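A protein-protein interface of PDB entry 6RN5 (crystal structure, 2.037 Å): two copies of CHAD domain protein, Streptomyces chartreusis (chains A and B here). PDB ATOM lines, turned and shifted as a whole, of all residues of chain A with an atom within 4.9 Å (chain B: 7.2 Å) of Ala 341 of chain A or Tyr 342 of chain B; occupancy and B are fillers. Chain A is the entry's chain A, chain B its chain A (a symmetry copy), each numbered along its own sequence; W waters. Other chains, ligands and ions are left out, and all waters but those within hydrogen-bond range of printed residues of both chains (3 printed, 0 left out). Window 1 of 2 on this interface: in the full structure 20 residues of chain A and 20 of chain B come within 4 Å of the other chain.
OH of Tyr 342 of chain A sits close to ND1 of His 348 of chain B (3.5 Å).
OH of Tyr 342 of chain B sits close to ND1 of His 348 of chain A.
The backbone carbonyl oxygen (O) of Leu 260 of chain A lies within hydrogen-bond range of a ring nitrogen (ND1) of His 348 of chain A (3.5 Å).
CB of Leu 260 of chain A touches CG1 of Val 346 of chain B, at 3.9 Å.
CB of Ala 328 of chain A touches OH of Tyr 342 of chain B, 3.7 Å away.
Pro 338 of chain B touches Ile 336 of chain A (CG to O, 3.7 Å).
CB of Ala 341 of chain B touches O of Pro 338 of chain A, at 3.3 Å.
CB of Ala 341 of chain A touches O of Pro 338 of chain B, 3.3 Å away.
O of Ala 341 of chain A touches CD2 of Tyr 342 of chain B, 3.4 Å away.
Tyr 342 of chain A touches Gly 345 of chain B (CD2 to N, 3.3 Å).
Tyr 342 of chain B touches Leu 344 of chain A.
Gly 345 of chain A touches Tyr 342 of chain B.
O of Gly 345 of chain A touches CG2 of Val 346 of chain B, 3.5 Å away.
Ala 341 of chain A touches just these residues of chain B: Pro 338 (3.3 Å) and Tyr 342 (3.4 Å).
Ala 343 of chain A touches none of the printed residues of chain B.
Of the printed residues of chain A, Ala 331 of chain B touches Tyr 342.
Ala 339 of chain B touches none of the printed residues of chain A.
Printed residues of chain A within 4 Å of Ala 341 of chain B: Pro 338 and Tyr 342.
Of chain A, only Ala 328 (3.7 Å), Ala 331 (3.5 Å), Ala 341 (3.4 Å), Leu 344 (3.8 Å), Gly 345 (3.3 Å) and His 348 (3.2 Å) come within 4 Å of Tyr 342 of chain B.
The nearest residue of chain B that does not touch Ala 341 of chain A is Ala 341 of chain B (4.5 Å).
The nearest printed residue of chain A that does not touch Tyr 342 of chain B is Tyr 342 of chain A (4.1 Å).
Of the 16 printed residues of chain A, 11 touch a printed residue of chain B.
Printed residues of chain A that touch a printed residue of chain B: Leu 260, Ile 261, Ala 328, Ala 331, Ile 336, Pro 338, Ala 341, Tyr 342, Leu 344, Gly 345 and His 348.
Hydrophobic or aromatic side chains of chain A within 4 Å of the printed part of chain B: Leu 260, Ile 261, Ala 328, Ala 331, Pro 338, Ala 341, Tyr 342 and His 348.
Printed residues of chain B that touch a printed residue of chain A: Ala 331, Ile 336, Pro 338, Ala 341, Tyr 342, Ala 343, Leu 344, Gly 345, Val 346 and His 348.
Among the printed residues, no Asp or Glu carboxylate lies within 4 Å of a Lys or Arg side-chain nitrogen of the other chain.
Ile 336 of chain A touches Pro 338 of chain B, and with the chains exchanged Pro 338 of chain A touches Ile 336 of chain B.
Ala 341 of chain A touches Tyr 342 of chain B, and with the chains exchanged Tyr 342 of chain A touches Ala 341 of chain B.
Tyr 342 of chain A touches Gly 345 of chain B, and with the chains exchanged Gly 345 of chain A touches Tyr 342 of chain B.
Tyr 342 of chain A touches His 348 of chain B, and with the chains exchanged His 348 of chain A touches Tyr 342 of chain B.
Of the 19 pairs that touch across the chains among the printed residues, 14 have their exchanged pair printed and touching as well.
Water W2 lies within hydrogen-bond range of OH of Tyr 342 of chain B (2.7 Å) and O of Leu 260 of chain A (3.1 Å).
Water W3 lies within hydrogen-bond range of O of Ala 331 of chain A and N of Ala 339 of chain B.
Water W1 bridges O of Ala 331 of chain B and N of Ala 339 of chain A.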
ATOM      1  N   LEU A 260      -8.177  -8.672   7.137  1.00  0.00           N
ATOM      2  CA  LEU A 260      -8.142 -10.100   7.354  1.00  0.00           C
ATOM      3  C   LEU A 260      -8.496 -10.499   8.782  1.00  0.00           C
ATOM      4  O   LEU A 260      -8.947 -11.610   9.032  1.00  0.00           O
ATOM      5  CB  LEU A 260      -6.778 -10.627   6.949  1.00  0.00           C
ATOM      6  CG  LEU A 260      -6.433 -10.264   5.511  1.00  0.00           C
ATOM      7  CD1 LEU A 260      -5.009 -10.664   5.175  1.00  0.00           C
ATOM      8  CD2 LEU A 260      -7.406 -10.926   4.549  1.00  0.00           C
ATOM      9  N   ILE A 261      -8.346  -9.599   9.724  1.00  0.00           N
ATOM     10  CA  ILE A 261      -8.834  -9.862  11.056  1.00  0.00           C
ATOM     11  C   ILE A 261      -9.836  -8.768  11.324  1.00  0.00           C
ATOM     12  O   ILE A 261      -9.484  -7.599  11.317  1.00  0.00           O
ATOM     13  CB  ILE A 261      -7.713  -9.815  12.108  1.00  0.00           C
ATOM     14  CG1 ILE A 261      -6.511 -10.660  11.693  1.00  0.00           C
ATOM     15  CG2 ILE A 261      -8.241 -10.362  13.421  1.00  0.00           C
ATOM     16  CD1 ILE A 261      -5.269 -10.420  12.548  1.00  0.00           C
ATOM     17  N   ALA A 327     -16.251 -19.079   6.755  1.00  0.00           N
ATOM     18  CA  ALA A 327     -15.144 -19.433   7.641  1.00  0.00           C
ATOM     19  C   ALA A 327     -15.120 -18.522   8.865  1.00  0.00           C
ATOM     20  O   ALA A 327     -14.942 -18.992   9.985  1.00  0.00           O
ATOM     21  CB  ALA A 327     -13.833 -19.338   6.901  1.00  0.00           C
ATOM     22  N   ALA A 328     -15.297 -17.222   8.644  1.00  0.00           N
ATOM     23  CA  ALA A 328     -15.300 -16.271   9.754  1.00  0.00           C
ATOM     24  C   ALA A 328     -16.426 -16.615  10.737  1.00  0.00           C
ATOM     25  O   ALA A 328     -16.205 -16.725  11.948  1.00  0.00           O
ATOM     26  CB  ALA A 328     -15.401 -14.808   9.263  1.00  0.00           C
ATOM     27  N   ALA A 331     -15.854 -19.587  12.882  1.00  0.00           N
ATOM     28  CA  ALA A 331     -14.912 -19.285  13.951  1.00  0.00           C
ATOM     29  C   ALA A 331     -15.571 -18.681  15.191  1.00  0.00           C
ATOM     30  O   ALA A 331     -14.969 -18.696  16.255  1.00  0.00           O
ATOM     31  CB  ALA A 331     -13.840 -18.325  13.428  1.00  0.00           C
ATOM     32  N   ILE A 336     -15.469 -23.976  20.268  1.00  0.00           N
ATOM     33  CA  ILE A 336     -14.489 -24.606  19.411  1.00  0.00           C
ATOM     34  C   ILE A 336     -13.125 -24.430  20.019  1.00  0.00           C
ATOM     35  O   ILE A 336     -12.875 -23.466  20.734  1.00  0.00           O
ATOM     36  CB  ILE A 336     -14.511 -24.096  17.961  1.00  0.00           C
ATOM     37  CG1 ILE A 336     -14.298 -22.562  17.902  1.00  0.00           C
ATOM     38  CG2 ILE A 336     -15.812 -24.569  17.315  1.00  0.00           C
ATOM     39  CD1 ILE A 336     -14.182 -22.039  16.487  1.00  0.00           C
ATOM     40  N   ALA A 337     -12.261 -25.394  19.714  1.00  0.00           N
ATOM     41  CA  ALA A 337     -10.851 -25.395  20.155  1.00  0.00           C
ATOM     42  C   ALA A 337     -10.061 -24.260  19.455  1.00  0.00           C
ATOM     43  O   ALA A 337     -10.398 -23.902  18.346  1.00  0.00           O
ATOM     44  CB  ALA A 337     -10.223 -26.758  19.815  1.00  0.00           C
ATOM     45  N   PRO A 338      -9.022 -23.698  20.111  1.00  0.00           N
ATOM     46  CA  PRO A 338      -8.162 -22.683  19.493  1.00  0.00           C
ATOM     47  C   PRO A 338      -7.565 -23.139  18.148  1.00  0.00           C
ATOM     48  O   PRO A 338      -7.496 -22.354  17.225  1.00  0.00           O
ATOM     49  CB  PRO A 338      -7.057 -22.480  20.531  1.00  0.00           C
ATOM     50  CG  PRO A 338      -7.784 -22.710  21.827  1.00  0.00           C
ATOM     51  CD  PRO A 338      -8.674 -23.898  21.530  1.00  0.00           C
ATOM     52  N   ALA A 339      -7.142 -24.395  18.053  1.00  0.00           N
ATOM     53  CA  ALA A 339      -6.556 -24.893  16.843  1.00  0.00           C
ATOM     54  C   ALA A 339      -7.567 -24.845  15.683  1.00  0.00           C
ATOM     55  O   ALA A 339      -7.203 -24.625  14.528  1.00  0.00           O
ATOM     56  CB  ALA A 339      -6.043 -26.313  17.064  1.00  0.00           C
ATOM     57  N   THR A 340      -8.847 -25.046  16.007  1.00  0.00           N
ATOM     58  CA  THR A 340      -9.891 -25.020  14.995  1.00  0.00           C
ATOM     59  C   THR A 340     -10.090 -23.576  14.526  1.00  0.00           C
ATOM     60  O   THR A 340     -10.118 -23.306  13.341  1.00  0.00           O
ATOM     61  CB  THR A 340     -11.170 -25.611  15.589  1.00  0.00           C
ATOM     62  OG1 THR A 340     -10.887 -26.956  15.976  1.00  0.00           O
ATOM     63  CG2 THR A 340     -12.291 -25.603  14.579  1.00  0.00           C
ATOM     64  N   ALA A 341     -10.165 -22.637  15.463  1.00  0.00           N
ATOM     65  CA  ALA A 341     -10.314 -21.236  15.095  1.00  0.00           C
ATOM     66  C   ALA A 341      -9.102 -20.738  14.306  1.00  0.00           C
ATOM     67  O   ALA A 341      -9.201 -19.884  13.424  1.00  0.00           O
ATOM     68  CB  ALA A 341     -10.518 -20.419  16.347  1.00  0.00           C
ATOM     69  N   TYR A 342      -7.944 -21.270  14.627  1.00  0.00           N
ATOM     70  CA  TYR A 342      -6.718 -20.843  13.961  1.00  0.00           C
ATOM     71  C   TYR A 342      -6.770 -21.277  12.540  1.00  0.00           C
ATOM     72  O   TYR A 342      -6.474 -20.502  11.664  1.00  0.00           O
ATOM     73  CB  TYR A 342      -5.534 -21.451  14.709  1.00  0.00           C
ATOM     74  CG  TYR A 342      -4.131 -21.293  14.125  1.00  0.00           C
ATOM     75  CD1 TYR A 342      -3.681 -22.122  13.074  1.00  0.00           C
ATOM     76  CD2 TYR A 342      -3.236 -20.406  14.699  1.00  0.00           C
ATOM     77  CE1 TYR A 342      -2.385 -22.013  12.593  1.00  0.00           C
ATOM     78  CE2 TYR A 342      -1.935 -20.295  14.242  1.00  0.00           C
ATOM     79  CZ  TYR A 342      -1.515 -21.105  13.204  1.00  0.00           C
ATOM     80  OH  TYR A 342      -0.245 -20.959  12.762  1.00  0.00           O
ATOM     81  N   ALA A 343      -7.206 -22.508  12.286  1.00  0.00           N
ATOM     82  CA  ALA A 343      -7.343 -22.958  10.933  1.00  0.00           C
ATOM     83  C   ALA A 343      -8.336 -22.114  10.137  1.00  0.00           C
ATOM     84  O   ALA A 343      -8.129 -21.844   8.962  1.00  0.00           O
ATOM     85  CB  ALA A 343      -7.787 -24.413  10.894  1.00  0.00           C
ATOM     86  N   LEU A 344      -9.439 -21.755  10.775  1.00  0.00           N
ATOM     87  CA  LEU A 344     -10.459 -20.990  10.136  1.00  0.00           C
ATOM     88  C   LEU A 344      -9.975 -19.598   9.815  1.00  0.00           C
ATOM     89  O   LEU A 344     -10.375 -19.049   8.808  1.00  0.00           O
ATOM     90  CB  LEU A 344     -11.698 -20.920  11.033  1.00  0.00           C
ATOM     91  CG  LEU A 344     -12.424 -22.242  11.240  1.00  0.00           C
ATOM     92  CD1 LEU A 344     -13.472 -22.050  12.334  1.00  0.00           C
ATOM     93  CD2 LEU A 344     -13.083 -22.660   9.950  1.00  0.00           C
ATOM     94  N   GLY A 345      -9.136 -19.020  10.669  1.00  0.00           N
ATOM     95  CA  GLY A 345      -8.460 -17.741  10.342  1.00  0.00           C
ATOM     96  C   GLY A 345      -7.652 -17.762   9.039  1.00  0.00           C
ATOM     97  O   GLY A 345      -7.708 -16.821   8.242  1.00  0.00           O
ATOM     98  N   HIS A 348     -10.210 -18.147   6.025  1.00  0.00           N
ATOM     99  CA  HIS A 348     -10.786 -16.851   5.695  1.00  0.00           C
ATOM    100  C   HIS A 348      -9.817 -15.995   4.914  1.00  0.00           C
ATOM    101  O   HIS A 348     -10.207 -15.374   3.929  1.00  0.00           O
ATOM    102  CB  HIS A 348     -11.234 -16.116   6.962  1.00  0.00           C
ATOM    103  CG  HIS A 348     -11.632 -14.689   6.728  1.00  0.00           C
ATOM    104  ND1 HIS A 348     -10.733 -13.648   6.817  1.00  0.00           N
ATOM    105  CD2 HIS A 348     -12.828 -14.135   6.396  1.00  0.00           C
ATOM    106  CE1 HIS A 348     -11.372 -12.507   6.564  1.00  0.00           C
ATOM    107  NE2 HIS A 348     -12.641 -12.783   6.295  1.00  0.00           N
ATOM    108  N   GLY B 171      -9.927  -9.812  18.738  1.00  0.00           N
ATOM    109  CA  GLY B 171      -9.031 -10.922  18.394  1.00  0.00           C
ATOM    110  C   GLY B 171      -7.582 -10.486  18.221  1.00  0.00           C
ATOM    111  O   GLY B 171      -6.671 -11.053  18.842  1.00  0.00           O
ATOM    112  N   ALA B 172      -7.404  -9.483  17.365  1.00  0.00           N
ATOM    113  CA  ALA B 172      -6.147  -8.864  17.107  1.00  0.00           C
ATOM    114  C   ALA B 172      -5.548  -8.238  18.352  1.00  0.00           C
ATOM    115  O   ALA B 172      -4.329  -8.295  18.539  1.00  0.00           O
ATOM    116  CB  ALA B 172      -6.330  -7.777  16.069  1.00  0.00           C
ATOM    117  N   ALA B 175      -4.410 -10.894  20.646  1.00  0.00           N
ATOM    118  CA  ALA B 175      -3.209 -11.575  20.153  1.00  0.00           C
ATOM    119  C   ALA B 175      -2.011 -10.691  20.413  1.00  0.00           C
ATOM    120  O   ALA B 175      -0.957 -11.178  20.769  1.00  0.00           O
ATOM    121  CB  ALA B 175      -3.301 -11.897  18.665  1.00  0.00           C
ATOM    122  N   ALA B 331      -0.309 -19.504  19.585  1.00  0.00           N
ATOM    123  CA  ALA B 331      -1.622 -20.100  19.380  1.00  0.00           C
ATOM    124  C   ALA B 331      -1.832 -21.394  20.166  1.00  0.00           C
ATOM    125  O   ALA B 331      -2.970 -21.804  20.349  1.00  0.00           O
ATOM    126  CB  ALA B 331      -1.829 -20.374  17.888  1.00  0.00           C
ATOM    127  N   ILE B 336      -6.450 -19.681  25.603  1.00  0.00           N
ATOM    128  CA  ILE B 336      -6.728 -18.494  24.825  1.00  0.00           C
ATOM    129  C   ILE B 336      -8.067 -18.650  24.160  1.00  0.00           C
ATOM    130  O   ILE B 336      -8.501 -19.760  23.874  1.00  0.00           O
ATOM    131  CB  ILE B 336      -5.639 -18.158  23.793  1.00  0.00           C
ATOM    132  CG1 ILE B 336      -5.408 -19.339  22.816  1.00  0.00           C
ATOM    133  CG2 ILE B 336      -4.387 -17.724  24.552  1.00  0.00           C
ATOM    134  CD1 ILE B 336      -4.439 -19.002  21.704  1.00  0.00           C
ATOM    135  N   ALA B 337      -8.701 -17.504  23.930  1.00  0.00           N
ATOM    136  CA  ALA B 337     -10.003 -17.416  23.237  1.00  0.00           C
ATOM    137  C   ALA B 337      -9.851 -17.805  21.744  1.00  0.00           C
ATOM    138  O   ALA B 337      -8.797 -17.593  21.182  1.00  0.00           O
ATOM    139  CB  ALA B 337     -10.535 -15.978  23.353  1.00  0.00           C
ATOM    140  N   PRO B 338     -10.903 -18.376  21.116  1.00  0.00           N
ATOM    141  CA  PRO B 338     -10.882 -18.693  19.684  1.00  0.00           C
ATOM    142  C   PRO B 338     -10.524 -17.480  18.805  1.00  0.00           C
ATOM    143  O   PRO B 338      -9.787 -17.626  17.851  1.00  0.00           O
ATOM    144  CB  PRO B 338     -12.314 -19.155  19.407  1.00  0.00           C
ATOM    145  CG  PRO B 338     -12.701 -19.809  20.704  1.00  0.00           C
ATOM    146  CD  PRO B 338     -12.134 -18.877  21.754  1.00  0.00           C
ATOM    147  N   ALA B 339     -11.047 -16.303  19.132  1.00  0.00           N
ATOM    148  CA  ALA B 339     -10.780 -15.128  18.355  1.00  0.00           C
ATOM    149  C   ALA B 339      -9.279 -14.788  18.374  1.00  0.00           C
ATOM    150  O   ALA B 339      -8.727 -14.281  17.396  1.00  0.00           O
ATOM    151  CB  ALA B 339     -11.612 -13.962  18.879  1.00  0.00           C
ATOM    152  N   THR B 340      -8.621 -15.080  19.499  1.00  0.00           N
ATOM    153  CA  THR B 340      -7.199 -14.806  19.630  1.00  0.00           C
ATOM    154  C   THR B 340      -6.421 -15.791  18.753  1.00  0.00           C
ATOM    155  O   THR B 340      -5.559 -15.399  17.992  1.00  0.00           O
ATOM    156  CB  THR B 340      -6.808 -14.919  21.104  1.00  0.00           C
ATOM    157  OG1 THR B 340      -7.568 -13.953  21.829  1.00  0.00           O
ATOM    158  CG2 THR B 340      -5.336 -14.649  21.296  1.00  0.00           C
ATOM    159  N   ALA B 341      -6.776 -17.071  18.815  1.00  0.00           N
ATOM    160  CA  ALA B 341      -6.111 -18.062  17.981  1.00  0.00           C
ATOM    161  C   ALA B 341      -6.345 -17.786  16.495  1.00  0.00           C
ATOM    162  O   ALA B 341      -5.500 -18.048  15.638  1.00  0.00           O
ATOM    163  CB  ALA B 341      -6.608 -19.435  18.361  1.00  0.00           C
ATOM    164  N   TYR B 342      -7.507 -17.257  16.182  1.00  0.00           N
ATOM    165  CA  TYR B 342      -7.849 -16.983  14.790  1.00  0.00           C
ATOM    166  C   TYR B 342      -6.972 -15.893  14.287  1.00  0.00           C
ATOM    167  O   TYR B 342      -6.431 -16.005  13.215  1.00  0.00           O
ATOM    168  CB  TYR B 342      -9.328 -16.609  14.730  1.00  0.00           C
ATOM    169  CG  TYR B 342      -9.913 -16.117  13.406  1.00  0.00           C
ATOM    170  CD1 TYR B 342      -9.727 -14.783  12.977  1.00  0.00           C
ATOM    171  CD2 TYR B 342     -10.733 -16.945  12.658  1.00  0.00           C
ATOM    172  CE1 TYR B 342     -10.313 -14.330  11.805  1.00  0.00           C
ATOM    173  CE2 TYR B 342     -11.338 -16.504  11.495  1.00  0.00           C
ATOM    174  CZ  TYR B 342     -11.136 -15.200  11.084  1.00  0.00           C
ATOM    175  OH  TYR B 342     -11.721 -14.803   9.932  1.00  0.00           O
ATOM    176  N   ALA B 343      -6.768 -14.847  15.084  1.00  0.00           N
ATOM    177  CA  ALA B 343      -5.877 -13.799  14.681  1.00  0.00           C
ATOM    178  C   ALA B 343      -4.450 -14.299  14.467  1.00  0.00           C
ATOM    179  O   ALA B 343      -3.762 -13.859  13.557  1.00  0.00           O
ATOM    180  CB  ALA B 343      -5.862 -12.683  15.716  1.00  0.00           C
ATOM    181  N   LEU B 344      -4.001 -15.176  15.351  1.00  0.00           N
ATOM    182  CA  LEU B 344      -2.676 -15.700  15.280  1.00  0.00           C
ATOM    183  C   LEU B 344      -2.498 -16.566  14.058  1.00  0.00           C
ATOM    184  O   LEU B 344      -1.422 -16.580  13.493  1.00  0.00           O
ATOM    185  CB  LEU B 344      -2.365 -16.506  16.544  1.00  0.00           C
ATOM    186  CG  LEU B 344      -2.280 -15.691  17.827  1.00  0.00           C
ATOM    187  CD1 LEU B 344      -2.208 -16.658  19.008  1.00  0.00           C
ATOM    188  CD2 LEU B 344      -1.049 -14.820  17.787  1.00  0.00           C
ATOM    189  N   GLY B 345      -3.533 -17.300  13.661  1.00  0.00           N
ATOM    190  CA  GLY B 345      -3.514 -18.027  12.368  1.00  0.00           C
ATOM    191  C   GLY B 345      -3.237 -17.145  11.145  1.00  0.00           C
ATOM    192  O   GLY B 345      -2.458 -17.514  10.260  1.00  0.00           O
ATOM    193  N   VAL B 346      -3.875 -15.974  11.121  1.00  0.00           N
ATOM    194  CA  VAL B 346      -3.715 -15.017  10.056  1.00  0.00           C
ATOM    195  C   VAL B 346      -2.292 -14.476  10.050  1.00  0.00           C
ATOM    196  O   VAL B 346      -1.637 -14.356   9.010  1.00  0.00           O
ATOM    197  CB  VAL B 346      -4.693 -13.828  10.245  1.00  0.00           C
ATOM    198  CG1 VAL B 346      -4.498 -12.782   9.181  1.00  0.00           C
ATOM    199  CG2 VAL B 346      -6.139 -14.304  10.151  1.00  0.00           C
ATOM    200  N   LEU B 347      -1.825 -14.142  11.244  1.00  0.00           N
ATOM    201  CA  LEU B 347      -0.488 -13.594  11.433  1.00  0.00           C
ATOM    202  C   LEU B 347       0.640 -14.564  11.058  1.00  0.00           C
ATOM    203  O   LEU B 347       1.622 -14.177  10.474  1.00  0.00           O
ATOM    204  CB  LEU B 347      -0.368 -13.170  12.877  1.00  0.00           C
ATOM    205  CG  LEU B 347       0.873 -12.484  13.342  1.00  0.00           C
ATOM    206  CD1 LEU B 347       1.091 -11.224  12.519  1.00  0.00           C
ATOM    207  CD2 LEU B 347       0.647 -12.172  14.817  1.00  0.00           C
ATOM    208  N   HIS B 348       0.500 -15.825  11.414  1.00  0.00           N
ATOM    209  CA  HIS B 348       1.422 -16.847  10.938  1.00  0.00           C
ATOM    210  C   HIS B 348       1.436 -16.924   9.430  1.00  0.00           C
ATOM    211  O   HIS B 348       2.505 -17.005   8.832  1.00  0.00           O
ATOM    212  CB  HIS B 348       1.071 -18.215  11.531  1.00  0.00           C
ATOM    213  CG  HIS B 348       1.832 -19.355  10.920  1.00  0.00           C
ATOM    214  ND1 HIS B 348       1.364 -20.055   9.829  1.00  0.00           N
ATOM    215  CD2 HIS B 348       3.033 -19.905  11.241  1.00  0.00           C
ATOM    216  CE1 HIS B 348       2.245 -21.003   9.517  1.00  0.00           C
ATOM    217  NE2 HIS B 348       3.270 -20.921  10.355  1.00  0.00           N
HETATM  218  O   HOH W   1      -4.020 -23.823  18.687  1.00  0.00           O
HETATM  219  O   HOH W   2     -11.920 -12.149   9.884  1.00  0.00           O
HETATM  220  O   HOH W   3     -13.574 -16.403  17.112  1.00  0.00           O
